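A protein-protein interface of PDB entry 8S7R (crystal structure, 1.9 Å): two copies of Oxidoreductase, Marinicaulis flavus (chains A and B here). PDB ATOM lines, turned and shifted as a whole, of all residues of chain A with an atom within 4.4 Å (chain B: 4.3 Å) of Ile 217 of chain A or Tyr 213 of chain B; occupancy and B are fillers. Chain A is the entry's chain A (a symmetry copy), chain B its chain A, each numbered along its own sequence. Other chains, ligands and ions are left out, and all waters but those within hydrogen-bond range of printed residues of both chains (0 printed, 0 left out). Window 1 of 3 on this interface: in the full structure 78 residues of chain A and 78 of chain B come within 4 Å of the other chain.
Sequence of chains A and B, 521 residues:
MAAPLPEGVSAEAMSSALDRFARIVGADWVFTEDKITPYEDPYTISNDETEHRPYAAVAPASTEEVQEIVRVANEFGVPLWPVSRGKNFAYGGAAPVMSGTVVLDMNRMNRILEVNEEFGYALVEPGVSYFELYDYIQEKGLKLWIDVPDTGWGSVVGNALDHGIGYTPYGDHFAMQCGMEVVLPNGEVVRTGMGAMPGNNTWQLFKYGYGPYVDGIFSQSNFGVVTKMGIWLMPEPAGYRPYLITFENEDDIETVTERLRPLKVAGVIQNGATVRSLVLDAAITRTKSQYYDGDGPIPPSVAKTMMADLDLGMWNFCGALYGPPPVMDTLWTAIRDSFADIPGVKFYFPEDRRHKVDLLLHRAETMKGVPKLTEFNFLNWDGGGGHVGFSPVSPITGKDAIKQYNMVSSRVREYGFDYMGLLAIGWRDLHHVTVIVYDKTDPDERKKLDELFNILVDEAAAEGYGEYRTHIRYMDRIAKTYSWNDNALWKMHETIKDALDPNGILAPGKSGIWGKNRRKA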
ATOM      1  N   VAL A 214     -19.932  15.930  21.886  1.00  0.00           N
ATOM      2  CA  VAL A 214     -21.185  15.200  21.737  1.00  0.00           C
ATOM      3  C   VAL A 214     -21.264  13.901  22.548  1.00  0.00           C
ATOM      4  O   VAL A 214     -22.323  13.284  22.563  1.00  0.00           O
ATOM      5  CB  VAL A 214     -21.488  14.915  20.258  1.00  0.00           C
ATOM      6  CG1 VAL A 214     -21.773  16.204  19.501  1.00  0.00           C
ATOM      7  CG2 VAL A 214     -20.406  14.065  19.606  1.00  0.00           C
ATOM      8  N   ASP A 215     -20.191  13.441  23.198  1.00  0.00           N
ATOM      9  CA  ASP A 215     -20.232  12.183  23.940  1.00  0.00           C
ATOM     10  C   ASP A 215     -21.425  12.146  24.894  1.00  0.00           C
ATOM     11  O   ASP A 215     -22.102  11.124  25.025  1.00  0.00           O
ATOM     12  CB  ASP A 215     -18.953  11.966  24.748  1.00  0.00           C
ATOM     13  CG  ASP A 215     -17.747  11.762  23.851  1.00  0.00           C
ATOM     14  OD1 ASP A 215     -17.423  12.708  23.098  1.00  0.00           O
ATOM     15  OD2 ASP A 215     -17.212  10.618  23.828  1.00  0.00           O
ATOM     16  N   GLY A 216     -21.645  13.273  25.581  1.00  0.00           N
ATOM     17  CA  GLY A 216     -22.698  13.414  26.574  1.00  0.00           C
ATOM     18  C   GLY A 216     -24.097  13.117  26.034  1.00  0.00           C
ATOM     19  O   GLY A 216     -24.960  12.707  26.791  1.00  0.00           O
ATOM     20  N   ILE A 217     -24.350  13.352  24.744  1.00  0.00           N
ATOM     21  CA  ILE A 217     -25.696  13.181  24.231  1.00  0.00           C
ATOM     22  C   ILE A 217     -26.077  11.701  24.116  1.00  0.00           C
ATOM     23  O   ILE A 217     -27.258  11.419  23.870  1.00  0.00           O
ATOM     24  CB  ILE A 217     -25.916  13.884  22.881  1.00  0.00           C
ATOM     25  CG1 ILE A 217     -25.395  13.060  21.690  1.00  0.00           C
ATOM     26  CG2 ILE A 217     -25.360  15.288  22.915  1.00  0.00           C
ATOM     27  CD1 ILE A 217     -25.792  13.631  20.357  1.00  0.00           C
ATOM     28  N   PHE A 218     -25.097  10.795  24.270  1.00  0.00           N
ATOM     29  CA  PHE A 218     -25.333   9.364  24.209  1.00  0.00           C
ATOM     30  C   PHE A 218     -25.421   8.780  25.617  1.00  0.00           C
ATOM     31  O   PHE A 218     -25.509   7.578  25.757  1.00  0.00           O
ATOM     32  CB  PHE A 218     -24.221   8.689  23.384  1.00  0.00           C
ATOM     33  CG  PHE A 218     -24.169   9.183  21.962  1.00  0.00           C
ATOM     34  CD1 PHE A 218     -25.230   8.950  21.098  1.00  0.00           C
ATOM     35  CD2 PHE A 218     -23.091   9.933  21.501  1.00  0.00           C
ATOM     36  CE1 PHE A 218     -25.217   9.463  19.803  1.00  0.00           C
ATOM     37  CE2 PHE A 218     -23.086  10.453  20.217  1.00  0.00           C
ATOM     38  CZ  PHE A 218     -24.138  10.213  19.364  1.00  0.00           C
ATOM     39  N   SER A 219     -25.390   9.623  26.647  1.00  0.00           N
ATOM     40  CA  SER A 219     -25.661   9.211  28.008  1.00  0.00           C
ATOM     41  C   SER A 219     -27.125   9.517  28.339  1.00  0.00           C
ATOM     42  O   SER A 219     -27.700  10.504  27.840  1.00  0.00           O
ATOM     43  CB  SER A 219     -24.704   9.886  28.969  1.00  0.00           C
ATOM     44  OG  SER A 219     -24.923  11.286  28.993  1.00  0.00           O
ATOM     45  N   SER A 221     -29.818   8.262  27.175  1.00  0.00           N
ATOM     46  CA  SER A 221     -30.268   8.712  25.872  1.00  0.00           C
ATOM     47  C   SER A 221     -30.748   7.550  25.006  1.00  0.00           C
ATOM     48  O   SER A 221     -30.382   6.412  25.237  1.00  0.00           O
ATOM     49  CB  SER A 221     -29.113   9.436  25.212  1.00  0.00           C
ATOM     50  OG  SER A 221     -29.389   9.768  23.878  1.00  0.00           O
ATOM     51  N   PHE A 223     -30.286   8.203  21.592  1.00  0.00           N
ATOM     52  CA  PHE A 223     -29.749   8.822  20.389  1.00  0.00           C
ATOM     53  C   PHE A 223     -28.760   7.911  19.650  1.00  0.00           C
ATOM     54  O   PHE A 223     -28.379   8.220  18.511  1.00  0.00           O
ATOM     55  CB  PHE A 223     -29.079  10.145  20.751  1.00  0.00           C
ATOM     56  CG  PHE A 223     -29.995  11.257  21.202  1.00  0.00           C
ATOM     57  CD1 PHE A 223     -31.374  11.178  21.073  1.00  0.00           C
ATOM     58  CD2 PHE A 223     -29.456  12.389  21.797  1.00  0.00           C
ATOM     59  CE1 PHE A 223     -32.178  12.220  21.514  1.00  0.00           C
ATOM     60  CE2 PHE A 223     -30.262  13.427  22.238  1.00  0.00           C
ATOM     61  CZ  PHE A 223     -31.622  13.350  22.082  1.00  0.00           C
ATOM     62  N   LYS B 207     -23.788  19.165  37.050  1.00  0.00           N
ATOM     63  CA  LYS B 207     -23.766  19.402  35.616  1.00  0.00           C
ATOM     64  C   LYS B 207     -24.944  18.780  34.879  1.00  0.00           C
ATOM     65  O   LYS B 207     -25.501  19.400  33.975  1.00  0.00           O
ATOM     66  CB  LYS B 207     -22.489  18.826  35.006  1.00  0.00           C
ATOM     67  CG  LYS B 207     -21.198  19.588  35.286  1.00  0.00           C
ATOM     68  CD  LYS B 207     -19.990  18.787  34.806  1.00  0.00           C
ATOM     69  CE  LYS B 207     -18.709  19.587  34.733  1.00  0.00           C
ATOM     70  NZ  LYS B 207     -18.678  20.382  33.481  1.00  0.00           N
ATOM     71  N   TYR B 208     -25.240  17.498  35.150  1.00  0.00           N
ATOM     72  CA  TYR B 208     -25.998  16.687  34.203  1.00  0.00           C
ATOM     73  C   TYR B 208     -27.462  17.095  34.064  1.00  0.00           C
ATOM     74  O   TYR B 208     -28.031  17.013  32.980  1.00  0.00           O
ATOM     75  CB  TYR B 208     -25.973  15.198  34.594  1.00  0.00           C
ATOM     76  CG  TYR B 208     -24.601  14.591  34.551  1.00  0.00           C
ATOM     77  CD1 TYR B 208     -23.745  14.808  33.475  1.00  0.00           C
ATOM     78  CD2 TYR B 208     -24.155  13.787  35.584  1.00  0.00           C
ATOM     79  CE1 TYR B 208     -22.462  14.273  33.457  1.00  0.00           C
ATOM     80  CE2 TYR B 208     -22.893  13.215  35.561  1.00  0.00           C
ATOM     81  CZ  TYR B 208     -22.041  13.453  34.497  1.00  0.00           C
ATOM     82  OH  TYR B 208     -20.781  12.870  34.543  1.00  0.00           O
ATOM     83  N   GLY B 211     -31.272  13.094  31.785  1.00  0.00           N
ATOM     84  CA  GLY B 211     -31.387  12.874  30.352  1.00  0.00           C
ATOM     85  C   GLY B 211     -30.069  13.177  29.642  1.00  0.00           C
ATOM     86  O   GLY B 211     -29.014  13.262  30.276  1.00  0.00           O
ATOM     87  N   PRO B 212     -30.101  13.310  28.301  1.00  0.00           N
ATOM     88  CA  PRO B 212     -28.894  13.539  27.519  1.00  0.00           C
ATOM     89  C   PRO B 212     -28.149  14.777  27.991  1.00  0.00           C
ATOM     90  O   PRO B 212     -28.741  15.818  28.278  1.00  0.00           O
ATOM     91  CB  PRO B 212     -29.392  13.727  26.085  1.00  0.00           C
ATOM     92  CG  PRO B 212     -30.795  13.143  26.059  1.00  0.00           C
ATOM     93  CD  PRO B 212     -31.312  13.267  27.479  1.00  0.00           C
ATOM     94  N   TYR B 213     -26.834  14.634  28.111  1.00  0.00           N
ATOM     95  CA  TYR B 213     -25.980  15.732  28.523  1.00  0.00           C
ATOM     96  C   TYR B 213     -25.565  16.532  27.282  1.00  0.00           C
ATOM     97  O   TYR B 213     -24.760  16.041  26.482  1.00  0.00           O
ATOM     98  CB  TYR B 213     -24.797  15.146  29.283  1.00  0.00           C
ATOM     99  CG  TYR B 213     -23.826  16.170  29.795  1.00  0.00           C
ATOM    100  CD1 TYR B 213     -24.265  17.346  30.370  1.00  0.00           C
ATOM    101  CD2 TYR B 213     -22.469  15.915  29.802  1.00  0.00           C
ATOM    102  CE1 TYR B 213     -23.373  18.275  30.875  1.00  0.00           C
ATOM    103  CE2 TYR B 213     -21.561  16.828  30.308  1.00  0.00           C
ATOM    104  CZ  TYR B 213     -22.014  18.024  30.826  1.00  0.00           C
ATOM    105  OH  TYR B 213     -21.110  18.943  31.302  1.00  0.00           O
ATOM    106  N   VAL B 214     -26.123  17.746  27.132  1.00  0.00           N
ATOM    107  CA  VAL B 214     -26.050  18.494  25.884  1.00  0.00           C
ATOM    108  C   VAL B 214     -25.220  19.782  25.963  1.00  0.00           C
ATOM    109  O   VAL B 214     -25.019  20.412  24.931  1.00  0.00           O
ATOM    110  CB  VAL B 214     -27.453  18.806  25.341  1.00  0.00           C
ATOM    111  CG1 VAL B 214     -28.167  17.532  24.912  1.00  0.00           C
ATOM    112  CG2 VAL B 214     -28.266  19.651  26.311  1.00  0.00           C
ATOM    113  N   ASP B 215     -24.754  20.218  27.136  1.00  0.00           N
ATOM    114  CA  ASP B 215     -24.000  21.465  27.240  1.00  0.00           C
ATOM    115  C   ASP B 215     -22.858  21.503  26.225  1.00  0.00           C
ATOM    116  O   ASP B 215     -22.601  22.531  25.596  1.00  0.00           O
ATOM    117  CB  ASP B 215     -23.416  21.653  28.640  1.00  0.00           C
ATOM    118  CG  ASP B 215     -24.501  21.854  29.681  1.00  0.00           C
ATOM    119  OD1 ASP B 215     -25.309  20.916  29.859  1.00  0.00           O
ATOM    120  OD2 ASP B 215     -24.598  22.992  30.222  1.00  0.00           O
ATOM    121  N   ILE B 217     -22.528  20.337  23.298  1.00  0.00           N
ATOM    122  CA  ILE B 217     -22.805  20.533  21.889  1.00  0.00           C
ATOM    123  C   ILE B 217     -22.835  22.020  21.516  1.00  0.00           C
ATOM    124  O   ILE B 217     -22.875  22.320  20.315  1.00  0.00           O
ATOM    125  CB  ILE B 217     -24.108  19.853  21.434  1.00  0.00           C
ATOM    126  CG1 ILE B 217     -25.358  20.689  21.759  1.00  0.00           C
ATOM    127  CG2 ILE B 217     -24.186  18.442  21.965  1.00  0.00           C
ATOM    128  CD1 ILE B 217     -26.613  20.144  21.134  1.00  0.00           C
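The backbone NH (N) of Tyr 213 of chain B lies within hydrogen-bond range of the backbone carbonyl oxygen (O) of Gly 216 of chain A, 3.0 Å away.
O of Tyr 213 of chain B sits at hydrogen-bond distance from N of Ile 217 of chain A (3.2 Å).
The side-chain hydroxyl (OG) of Ser 219 of chain A is in hydrogen-bond range of the backbone carbonyl oxygen (O) of Gly 216 of chain A.
O of Ile 217 of chain A lies within hydrogen-bond range of OG of Ser 221 of chain A, at 2.7 Å.
OG of Ser 221 of chain A lies within hydrogen-bond range of N of Phe 223 of chain A, 2.9 Å away.
Among the printed residues, pairs that only touch across the chains: Gly 216 of chain A with Pro 212 of chain B (3.99 Å), Ile 217 of chain A with Pro 212 of chain B (3.8 Å), Ile 217 of chain A with Ile 217 of chain B (3.5 Å), Ser 219 of chain A with Gly 211 of chain B (3.9 Å), Ser 219 of chain A with Pro 212 of chain B (3.3 Å), Ser 219 of chain A with Tyr 213 of chain B (3.9 Å) and Phe 223 of chain A with Pro 212 of chain B (3.9 Å).
Of chain A, only Gly 216 (3.0 Å), Ile 217 (3.2 Å) and Ser 219 (3.9 Å) come within 4 Å of Tyr 213 of chain B.
Printed residues of chain B within 4 Å of Gly 216 of chain A: Pro 212 and Tyr 213.
Printed residues of chain B within 4 Å of Ser 219 of chain A: Gly 211, Pro 212 and Tyr 213.
Printed residues of chain A within 4 Å of Gly 211 of chain B: Ser 219.
Printed residues of chain A within 4 Å of Ile 217 of chain B: Ile 217.
Printed residues of chain A within 4 Å of Pro 212 of chain B: Gly 216, Ile 217, Ser 219 and Phe 223.
The nearest residue of chain B that does not touch Ile 217 of chain A is Val 214 of chain B (4.1 Å).
The nearest printed residue of chain A that does not touch Tyr 213 of chain B is Asp 215 of chain A (5.4 Å).
Of the 8 printed residues of chain A, 4 touch a printed residue of chain B.
Hydrophobic or aromatic side chains of chain A within 4 Å of the printed part of chain B: Ile 217 and Phe 223.
Printed residues of chain B that touch a printed residue of chain A: Gly 211, Pro 212, Tyr 213 and Ile 217.
Hydrophobic or aromatic side chains of chain B that line the printed part of chain A: Pro 212, Tyr 213 and Ile 217.
Among the printed residues, no Asp or Glu carboxylate lies within 4 Å of a Lys or Arg side-chain nitrogen of the other chain.
Ile 217 of chain B touches its own counterpart, Ile 217 of chain A.
Positions printed for both chains: 214, 215 and 217.
Of the 9 pairs that touch across the chains among the printed residues, 1 has its exchanged pair printed and touching as well.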
